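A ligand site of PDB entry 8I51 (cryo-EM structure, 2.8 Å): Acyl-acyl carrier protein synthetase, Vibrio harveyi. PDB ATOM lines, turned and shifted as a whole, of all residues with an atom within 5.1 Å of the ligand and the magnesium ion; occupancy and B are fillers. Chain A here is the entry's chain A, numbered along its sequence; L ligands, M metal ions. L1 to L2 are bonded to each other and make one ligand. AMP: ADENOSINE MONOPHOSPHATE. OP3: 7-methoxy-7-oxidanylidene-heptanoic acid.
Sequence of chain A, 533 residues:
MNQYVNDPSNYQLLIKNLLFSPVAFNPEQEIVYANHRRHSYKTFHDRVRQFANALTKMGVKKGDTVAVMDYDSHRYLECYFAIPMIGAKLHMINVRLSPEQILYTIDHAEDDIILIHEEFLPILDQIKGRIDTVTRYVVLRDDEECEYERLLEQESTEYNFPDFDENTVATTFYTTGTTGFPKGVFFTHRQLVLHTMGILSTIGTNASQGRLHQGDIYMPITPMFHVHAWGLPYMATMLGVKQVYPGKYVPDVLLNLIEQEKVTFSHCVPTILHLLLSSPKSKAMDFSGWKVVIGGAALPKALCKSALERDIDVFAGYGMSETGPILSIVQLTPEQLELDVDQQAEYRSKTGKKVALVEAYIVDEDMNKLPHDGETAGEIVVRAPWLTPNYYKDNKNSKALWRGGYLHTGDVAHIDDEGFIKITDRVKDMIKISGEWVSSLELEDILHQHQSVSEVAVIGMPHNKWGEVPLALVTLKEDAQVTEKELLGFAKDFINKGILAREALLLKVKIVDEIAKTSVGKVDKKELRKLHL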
ATOM      1  N   THR A 175     -35.390  15.641 -10.607  1.00  0.00           N
ATOM      2  CA  THR A 175     -35.481  14.456 -11.466  1.00  0.00           C
ATOM      3  C   THR A 175     -36.679  13.590 -11.083  1.00  0.00           C
ATOM      4  O   THR A 175     -37.204  13.660  -9.976  1.00  0.00           O
ATOM      5  CB  THR A 175     -34.204  13.621 -11.369  1.00  0.00           C
ATOM      6  OG1 THR A 175     -34.275  12.534 -12.300  1.00  0.00           O
ATOM      7  CG2 THR A 175     -34.031  13.073  -9.962  1.00  0.00           C
ATOM      8  N   VAL A 227     -30.560  18.650 -17.062  1.00  0.00           N
ATOM      9  CA  VAL A 227     -29.538  18.832 -16.050  1.00  0.00           C
ATOM     10  C   VAL A 227     -28.484  19.809 -16.543  1.00  0.00           C
ATOM     11  O   VAL A 227     -27.559  19.438 -17.279  1.00  0.00           O
ATOM     12  CB  VAL A 227     -28.938  17.467 -15.634  1.00  0.00           C
ATOM     13  CG1 VAL A 227     -28.599  16.622 -16.855  1.00  0.00           C
ATOM     14  CG2 VAL A 227     -27.723  17.665 -14.730  1.00  0.00           C
ATOM     15  N   TRP A 230     -26.305  19.534 -19.498  1.00  0.00           N
ATOM     16  CA  TRP A 230     -25.092  18.745 -19.348  1.00  0.00           C
ATOM     17  C   TRP A 230     -23.873  19.592 -18.986  1.00  0.00           C
ATOM     18  O   TRP A 230     -22.739  19.213 -19.263  1.00  0.00           O
ATOM     19  CB  TRP A 230     -24.801  17.915 -20.613  1.00  0.00           C
ATOM     20  CG  TRP A 230     -25.948  17.029 -20.994  1.00  0.00           C
ATOM     21  CD1 TRP A 230     -26.999  16.669 -20.208  1.00  0.00           C
ATOM     22  CD2 TRP A 230     -26.141  16.377 -22.253  1.00  0.00           C
ATOM     23  NE1 TRP A 230     -27.852  15.844 -20.900  1.00  0.00           N
ATOM     24  CE2 TRP A 230     -27.341  15.647 -22.161  1.00  0.00           C
ATOM     25  CE3 TRP A 230     -25.432  16.333 -23.449  1.00  0.00           C
ATOM     26  CZ2 TRP A 230     -27.839  14.888 -23.216  1.00  0.00           C
ATOM     27  CZ3 TRP A 230     -25.925  15.586 -24.499  1.00  0.00           C
ATOM     28  CH2 TRP A 230     -27.119  14.871 -24.374  1.00  0.00           C
ATOM     29  N   VAL A 293     -22.336  15.340 -29.348  1.00  0.00           N
ATOM     30  CA  VAL A 293     -22.241  14.391 -28.275  1.00  0.00           C
ATOM     31  C   VAL A 293     -23.644  13.918 -27.948  1.00  0.00           C
ATOM     32  O   VAL A 293     -24.381  14.594 -27.297  1.00  0.00           O
ATOM     33  CB  VAL A 293     -21.531  14.870 -27.029  1.00  0.00           C
ATOM     34  CG1 VAL A 293     -22.227  16.029 -26.369  1.00  0.00           C
ATOM     35  CG2 VAL A 293     -21.158  13.756 -26.077  1.00  0.00           C
ATOM     36  N   GLY A 295     -25.528  11.947 -25.829  1.00  0.00           N
ATOM     37  CA  GLY A 295     -25.437  11.304 -24.541  1.00  0.00           C
ATOM     38  C   GLY A 295     -26.777  11.172 -23.843  1.00  0.00           C
ATOM     39  O   GLY A 295     -26.839  11.023 -22.627  1.00  0.00           O
ATOM     40  N   GLY A 296     -27.862  11.235 -24.616  1.00  0.00           N
ATOM     41  CA  GLY A 296     -29.185  11.131 -24.037  1.00  0.00           C
ATOM     42  C   GLY A 296     -29.463   9.761 -23.456  1.00  0.00           C
ATOM     43  O   GLY A 296     -29.555   9.616 -22.240  1.00  0.00           O
ATOM     44  N   ALA A 297     -29.612   8.760 -24.318  1.00  0.00           N
ATOM     45  CA  ALA A 297     -29.817   7.388 -23.861  1.00  0.00           C
ATOM     46  C   ALA A 297     -29.548   6.415 -25.004  1.00  0.00           C
ATOM     47  O   ALA A 297     -30.295   6.417 -25.987  1.00  0.00           O
ATOM     48  CB  ALA A 297     -31.234   7.198 -23.316  1.00  0.00           C
ATOM     49  N   ALA A 298     -28.511   5.598 -24.866  1.00  0.00           N
ATOM     50  CA  ALA A 298     -28.309   4.406 -25.691  1.00  0.00           C
ATOM     51  C   ALA A 298     -28.280   4.748 -27.183  1.00  0.00           C
ATOM     52  O   ALA A 298     -29.175   4.398 -27.955  1.00  0.00           O
ATOM     53  CB  ALA A 298     -29.381   3.349 -25.393  1.00  0.00           C
ATOM     54  N   ALA A 316     -20.629   9.269 -28.021  1.00  0.00           N
ATOM     55  CA  ALA A 316     -21.641   9.229 -26.982  1.00  0.00           C
ATOM     56  C   ALA A 316     -21.069   9.631 -25.636  1.00  0.00           C
ATOM     57  O   ALA A 316     -19.859   9.545 -25.385  1.00  0.00           O
ATOM     58  CB  ALA A 316     -22.261   7.837 -26.887  1.00  0.00           C
ATOM     59  N   GLY A 317     -21.963  10.080 -24.748  1.00  0.00           N
ATOM     60  CA  GLY A 317     -21.597  10.399 -23.390  1.00  0.00           C
ATOM     61  C   GLY A 317     -22.581   9.758 -22.425  1.00  0.00           C
ATOM     62  O   GLY A 317     -23.597   9.185 -22.832  1.00  0.00           O
ATOM     63  N   TYR A 318     -22.262   9.853 -21.134  1.00  0.00           N
ATOM     64  CA  TYR A 318     -23.084   9.210 -20.130  1.00  0.00           C
ATOM     65  C   TYR A 318     -23.031   9.963 -18.816  1.00  0.00           C
ATOM     66  O   TYR A 318     -21.943  10.276 -18.317  1.00  0.00           O
ATOM     67  CB  TYR A 318     -22.659   7.762 -19.905  1.00  0.00           C
ATOM     68  CG  TYR A 318     -23.358   7.137 -18.722  1.00  0.00           C
ATOM     69  CD1 TYR A 318     -24.727   6.934 -18.741  1.00  0.00           C
ATOM     70  CD2 TYR A 318     -22.656   6.787 -17.581  1.00  0.00           C
ATOM     71  CE1 TYR A 318     -25.377   6.386 -17.671  1.00  0.00           C
ATOM     72  CE2 TYR A 318     -23.310   6.229 -16.503  1.00  0.00           C
ATOM     73  CZ  TYR A 318     -24.666   6.024 -16.551  1.00  0.00           C
ATOM     74  OH  TYR A 318     -25.315   5.477 -15.481  1.00  0.00           O
ATOM     75  N   GLY A 319     -24.212  10.225 -18.264  1.00  0.00           N
ATOM     76  CA  GLY A 319     -24.401  10.813 -16.962  1.00  0.00           C
ATOM     77  C   GLY A 319     -25.872  10.760 -16.620  1.00  0.00           C
ATOM     78  O   GLY A 319     -26.703  10.365 -17.445  1.00  0.00           O
ATOM     79  N   MET A 320     -26.204  11.164 -15.402  1.00  0.00           N
ATOM     80  CA  MET A 320     -27.589  11.185 -14.952  1.00  0.00           C
ATOM     81  C   MET A 320     -27.823  12.431 -14.126  1.00  0.00           C
ATOM     82  O   MET A 320     -26.910  13.221 -13.868  1.00  0.00           O
ATOM     83  CB  MET A 320     -27.939   9.920 -14.162  1.00  0.00           C
ATOM     84  CG  MET A 320     -27.021   9.660 -12.984  1.00  0.00           C
ATOM     85  SD  MET A 320     -27.424   8.135 -12.135  1.00  0.00           S
ATOM     86  CE  MET A 320     -27.654   7.046 -13.531  1.00  0.00           C
ATOM     87  N   SER A 321     -29.074  12.611 -13.696  1.00  0.00           N
ATOM     88  CA  SER A 321     -29.466  13.821 -12.975  1.00  0.00           C
ATOM     89  C   SER A 321     -28.733  13.955 -11.646  1.00  0.00           C
ATOM     90  O   SER A 321     -28.515  15.073 -11.175  1.00  0.00           O
ATOM     91  CB  SER A 321     -30.971  13.827 -12.755  1.00  0.00           C
ATOM     92  OG  SER A 321     -31.664  13.634 -13.969  1.00  0.00           O
ATOM     93  N   GLU A 322     -28.364  12.838 -11.022  1.00  0.00           N
ATOM     94  CA  GLU A 322     -27.734  12.866  -9.711  1.00  0.00           C
ATOM     95  C   GLU A 322     -26.224  13.027  -9.769  1.00  0.00           C
ATOM     96  O   GLU A 322     -25.605  13.143  -8.705  1.00  0.00           O
ATOM     97  CB  GLU A 322     -28.074  11.580  -8.940  1.00  0.00           C
ATOM     98  CG  GLU A 322     -29.543  11.404  -8.603  1.00  0.00           C
ATOM     99  CD  GLU A 322     -30.313  10.698  -9.685  1.00  0.00           C
ATOM    100  OE1 GLU A 322     -29.708  10.354 -10.721  1.00  0.00           O
ATOM    101  OE2 GLU A 322     -31.530  10.479  -9.514  1.00  0.00           O
ATOM    102  N   PRO A 325     -24.108  16.394 -14.663  1.00  0.00           N
ATOM    103  CA  PRO A 325     -24.347  14.956 -14.875  1.00  0.00           C
ATOM    104  C   PRO A 325     -23.165  14.127 -15.361  1.00  0.00           C
ATOM    105  O   PRO A 325     -23.118  12.929 -15.073  1.00  0.00           O
ATOM    106  CB  PRO A 325     -25.449  14.977 -15.934  1.00  0.00           C
ATOM    107  CG  PRO A 325     -25.035  16.108 -16.822  1.00  0.00           C
ATOM    108  CD  PRO A 325     -24.382  17.138 -15.909  1.00  0.00           C
ATOM    109  N   ILE A 326     -22.211  14.701 -16.088  1.00  0.00           N
ATOM    110  CA  ILE A 326     -21.310  13.910 -16.921  1.00  0.00           C
ATOM    111  C   ILE A 326     -20.441  13.000 -16.064  1.00  0.00           C
ATOM    112  O   ILE A 326     -19.807  13.445 -15.104  1.00  0.00           O
ATOM    113  CB  ILE A 326     -20.450  14.837 -17.794  1.00  0.00           C
ATOM    114  CG1 ILE A 326     -21.330  15.843 -18.535  1.00  0.00           C
ATOM    115  CG2 ILE A 326     -19.644  14.006 -18.782  1.00  0.00           C
ATOM    116  CD1 ILE A 326     -20.594  16.648 -19.580  1.00  0.00           C
ATOM    117  N   SER A 328     -19.020   9.801 -17.997  1.00  0.00           N
ATOM    118  CA  SER A 328     -18.131   9.148 -18.941  1.00  0.00           C
ATOM    119  C   SER A 328     -18.355   9.741 -20.325  1.00  0.00           C
ATOM    120  O   SER A 328     -19.460  10.146 -20.667  1.00  0.00           O
ATOM    121  CB  SER A 328     -18.352   7.635 -18.978  1.00  0.00           C
ATOM    122  OG  SER A 328     -19.461   7.296 -19.794  1.00  0.00           O
ATOM    123  N   ILE A 329     -17.273   9.798 -21.111  1.00  0.00           N
ATOM    124  CA  ILE A 329     -17.320  10.306 -22.474  1.00  0.00           C
ATOM    125  C   ILE A 329     -16.467   9.417 -23.356  1.00  0.00           C
ATOM    126  O   ILE A 329     -15.377   8.995 -22.961  1.00  0.00           O
ATOM    127  CB  ILE A 329     -16.860  11.780 -22.561  1.00  0.00           C
ATOM    128  CG1 ILE A 329     -17.655  12.660 -21.602  1.00  0.00           C
ATOM    129  CG2 ILE A 329     -17.008  12.312 -23.974  1.00  0.00           C
ATOM    130  CD1 ILE A 329     -17.058  14.010 -21.368  1.00  0.00           C
ATOM    131  N   LYS A 350     -20.394   3.151 -27.539  1.00  0.00           N
ATOM    132  CA  LYS A 350     -20.272   2.626 -26.191  1.00  0.00           C
ATOM    133  C   LYS A 350     -20.563   3.713 -25.155  1.00  0.00           C
ATOM    134  O   LYS A 350     -20.814   4.872 -25.496  1.00  0.00           O
ATOM    135  CB  LYS A 350     -18.878   2.037 -25.975  1.00  0.00           C
ATOM    136  CG  LYS A 350     -18.636   0.714 -26.690  1.00  0.00           C
ATOM    137  CD  LYS A 350     -17.347   0.076 -26.221  1.00  0.00           C
ATOM    138  CE  LYS A 350     -17.200  -1.337 -26.770  1.00  0.00           C
ATOM    139  NZ  LYS A 350     -16.922  -1.331 -28.230  1.00  0.00           N
ATOM    140  N   THR A 351     -20.538   3.322 -23.886  1.00  0.00           N
ATOM    141  CA  THR A 351     -20.744   4.289 -22.808  1.00  0.00           C
ATOM    142  C   THR A 351     -19.515   5.178 -22.609  1.00  0.00           C
ATOM    143  O   THR A 351     -19.661   6.349 -22.248  1.00  0.00           O
ATOM    144  CB  THR A 351     -21.088   3.546 -21.514  1.00  0.00           C
ATOM    145  OG1 THR A 351     -22.200   2.676 -21.755  1.00  0.00           O
ATOM    146  CG2 THR A 351     -21.459   4.514 -20.409  1.00  0.00           C
ATOM    147  N   THR A 409     -25.986   4.231  -9.211  1.00  0.00           N
ATOM    148  CA  THR A 409     -26.501   4.703 -10.432  1.00  0.00           C
ATOM    149  C   THR A 409     -27.641   3.986 -10.865  1.00  0.00           C
ATOM    150  O   THR A 409     -28.565   4.522 -11.360  1.00  0.00           O
ATOM    151  CB  THR A 409     -25.363   4.527 -11.423  1.00  0.00           C
ATOM    152  OG1 THR A 409     -24.249   5.299 -10.997  1.00  0.00           O
ATOM    153  CG2 THR A 409     -25.689   4.847 -12.765  1.00  0.00           C
ATOM    154  N   ASP A 411     -27.687   1.309 -13.016  1.00  0.00           N
ATOM    155  CA  ASP A 411     -27.537   0.731 -14.340  1.00  0.00           C
ATOM    156  C   ASP A 411     -26.588  -0.465 -14.274  1.00  0.00           C
ATOM    157  O   ASP A 411     -25.561  -0.409 -13.601  1.00  0.00           O
ATOM    158  CB  ASP A 411     -27.008   1.756 -15.344  1.00  0.00           C
ATOM    159  CG  ASP A 411     -28.029   2.830 -15.669  1.00  0.00           C
ATOM    160  OD1 ASP A 411     -29.150   2.488 -16.106  1.00  0.00           O
ATOM    161  OD2 ASP A 411     -27.726   4.022 -15.468  1.00  0.00           O
ATOM    162  N   ILE A 423     -23.093  -0.077 -21.088  1.00  0.00           N
ATOM    163  CA  ILE A 423     -24.295  -0.249 -20.281  1.00  0.00           C
ATOM    164  C   ILE A 423     -25.180  -1.302 -20.933  1.00  0.00           C
ATOM    165  O   ILE A 423     -25.516  -1.211 -22.120  1.00  0.00           O
ATOM    166  CB  ILE A 423     -25.034   1.084 -20.109  1.00  0.00           C
ATOM    167  CG1 ILE A 423     -24.470   1.845 -18.913  1.00  0.00           C
ATOM    168  CG2 ILE A 423     -26.524   0.861 -19.928  1.00  0.00           C
ATOM    169  CD1 ILE A 423     -25.213   3.103 -18.601  1.00  0.00           C
ATOM    170  N   ARG A 426     -30.937  -2.027 -16.905  1.00  0.00           N
ATOM    171  CA  ARG A 426     -31.211  -1.264 -15.710  1.00  0.00           C
ATOM    172  C   ARG A 426     -31.363  -2.247 -14.659  1.00  0.00           C
ATOM    173  O   ARG A 426     -31.583  -3.371 -14.944  1.00  0.00           O
ATOM    174  CB  ARG A 426     -32.456  -0.461 -15.861  1.00  0.00           C
ATOM    175  CG  ARG A 426     -32.521   0.756 -14.980  1.00  0.00           C
ATOM    176  CD  ARG A 426     -32.315   2.069 -15.721  1.00  0.00           C
ATOM    177  NE  ARG A 426     -32.718   3.190 -14.880  1.00  0.00           N
ATOM    178  CZ  ARG A 426     -31.906   3.885 -14.097  1.00  0.00           C
ATOM    179  NH1 ARG A 426     -30.658   3.613 -14.064  1.00  0.00           N
ATOM    180  NH2 ARG A 426     -32.360   4.868 -13.363  1.00  0.00           N
HETATM  181  P   AMP L   1     -31.771  10.942 -15.988  1.00  0.00           P
HETATM  182  O1P AMP L   1     -31.700  10.435 -14.575  1.00  0.00           O
HETATM  183  O2P AMP L   1     -33.148  11.041 -16.578  1.00  0.00           O
HETATM  184  O3P AMP L   1     -30.942  12.156 -16.200  1.00  0.00           O
HETATM  185  O5' AMP L   1     -31.068   9.824 -16.882  1.00  0.00           O
HETATM  186  C5' AMP L   1     -30.622   8.641 -16.259  1.00  0.00           C
HETATM  187  C4' AMP L   1     -30.434   7.508 -17.241  1.00  0.00           C
HETATM  188  O4' AMP L   1     -30.027   7.892 -18.538  1.00  0.00           O
HETATM  189  C3' AMP L   1     -29.282   6.669 -16.826  1.00  0.00           C
HETATM  190  O3' AMP L   1     -29.626   5.825 -15.752  1.00  0.00           O
HETATM  191  C2' AMP L   1     -29.022   5.859 -18.049  1.00  0.00           C
HETATM  192  O2' AMP L   1     -29.726   4.615 -18.022  1.00  0.00           O
HETATM  193  C1' AMP L   1     -29.516   6.728 -19.177  1.00  0.00           C
HETATM  194  N9  AMP L   1     -28.369   7.015 -20.041  1.00  0.00           N
HETATM  195  C8  AMP L   1     -27.743   8.188 -20.169  1.00  0.00           C
HETATM  196  N7  AMP L   1     -26.740   8.101 -21.062  1.00  0.00           N
HETATM  197  C5  AMP L   1     -26.701   6.825 -21.498  1.00  0.00           C
HETATM  198  C6  AMP L   1     -25.866   6.051 -22.416  1.00  0.00           C
HETATM  199  N6  AMP L   1     -24.850   6.611 -23.114  1.00  0.00           N
HETATM  200  N1  AMP L   1     -26.165   4.742 -22.580  1.00  0.00           N
HETATM  201  C2  AMP L   1     -27.180   4.166 -21.922  1.00  0.00           C
HETATM  202  N3  AMP L   1     -27.966   4.818 -21.074  1.00  0.00           N
HETATM  203  C4  AMP L   1     -27.770   6.129 -20.814  1.00  0.00           C
HETATM  204  CAA OP3 L   2     -21.856  13.968 -22.262  1.00  0.00           C
HETATM  205  CAL OP3 L   2     -26.991  13.413 -18.850  1.00  0.00           C
HETATM  206  CAM OP3 L   2     -26.087  13.152 -20.043  1.00  0.00           C
HETATM  207  CAN OP3 L   2     -28.307  12.635 -18.933  1.00  0.00           C
HETATM  208  CAR OP3 L   2     -24.811  13.979 -19.994  1.00  0.00           C
HETATM  209  CAT OP3 L   2     -29.179  12.856 -17.700  1.00  0.00           C
HETATM  210  OAE OP3 L   2     -24.269  12.952 -22.040  1.00  0.00           O
HETATM  211  OAX OP3 L   2     -22.831  14.573 -21.465  1.00  0.00           O
HETATM  212  CBB OP3 L   2     -23.960  13.782 -21.245  1.00  0.00           C
HETATM  213  CBC OP3 L   2     -30.486  12.073 -17.761  1.00  0.00           C
HETATM  214  O25 OP3 L   2     -30.541  11.364 -18.967  1.00  0.00           O
HETATM  215 MG    MG M   1     -31.293   9.336 -12.798  1.00  0.00          MG
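A nitrogen (N6) of AMP L1 lies within hydrogen-bond range of the backbone carbonyl oxygen (O) of Gly 317 (2.9 Å).
An oxygen (O3') of AMP L1 sits at hydrogen-bond distance from the side-chain carboxylate of Asp 411, at 2.6 Å.
N of Ala 298 lies within hydrogen-bond range of N1 of AMP L1.
An oxygen (O3P) of AMP L1 lies within hydrogen-bond range of the side-chain hydroxyl of Ser 321 (2.8 Å).
N of Ser 321 sits at hydrogen-bond distance from O3P of AMP L1 (3.2 Å).
The guanidinium group (NH1) of Arg 426 lies within hydrogen-bond range of an oxygen (O3') of AMP L1, at 3.0 Å.
OD2 of Asp 411 lies within hydrogen-bond range of OH of Tyr 318 (2.8 Å).
The side-chain carboxylate of Asp 411 is in salt-bridge range of the guanidinium group of Arg 426 (2.8 Å).
The side-chain hydroxyl (OG1) of Thr 351 is in hydrogen-bond range of the backbone NH (N) of Ile 423, 3.0 Å away.
The backbone NH (N) of Tyr 318 is in hydrogen-bond range of the backbone carbonyl oxygen (O) of Ser 328.
The side-chain hydroxyl (OG) of Ser 321 lies within hydrogen-bond range of the side-chain hydroxyl (OG1) of Thr 175 (3.3 Å).
O of Gly 295 lies close to OAE of OP3 L2, 3.3 Å away.
O of Gly 296 lies close to N7 of AMP L1, at 3.4 Å.
Val 227 touches the ligand.
NE1 of Trp 230 touches CAL of OP3 L2, 3.3 Å away.
CG2 of Val 293 touches CAA of OP3 L2, 3.9 Å away.
Ala 297 touches the ligand.
CD1 of Tyr 318 touches N7 of AMP L1, at 3.3 Å.
O of Gly 319 touches CAN of OP3 L2 (3.2 Å).
Met 320 touches the ligand.
CB of Pro 325 touches CAL of OP3 L2 (3.7 Å).
CG1 of Ile 326 touches OAX of OP3 L2, at 3.5 Å.
CG2 of Ile 423 touches C2 of AMP L1, at 3.9 Å.
Hydrophobic or aromatic side chains within 4 Å of the ligand: Val 227, Trp 230, Val 293, Tyr 318, Met 320, Pro 325, Ile 326 and Ile 423.
Of the 25 residues printed, 17 come within 4 Å of the ligand.
CB of Met 320 touches the magnesium ion, at 3.7 Å.
Of the 25 residues printed, 2 come within 4 Å of the magnesium ion.
The nearest printed residue that does not touch the magnesium ion is Ser 321 (4.1 Å).
O1P of AMP L1 binds the magnesium ion, 2.1 Å away.
Slightly farther from the magnesium ion lies the side-chain carboxylate (OE1) of Glu 322 (2.8 Å).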
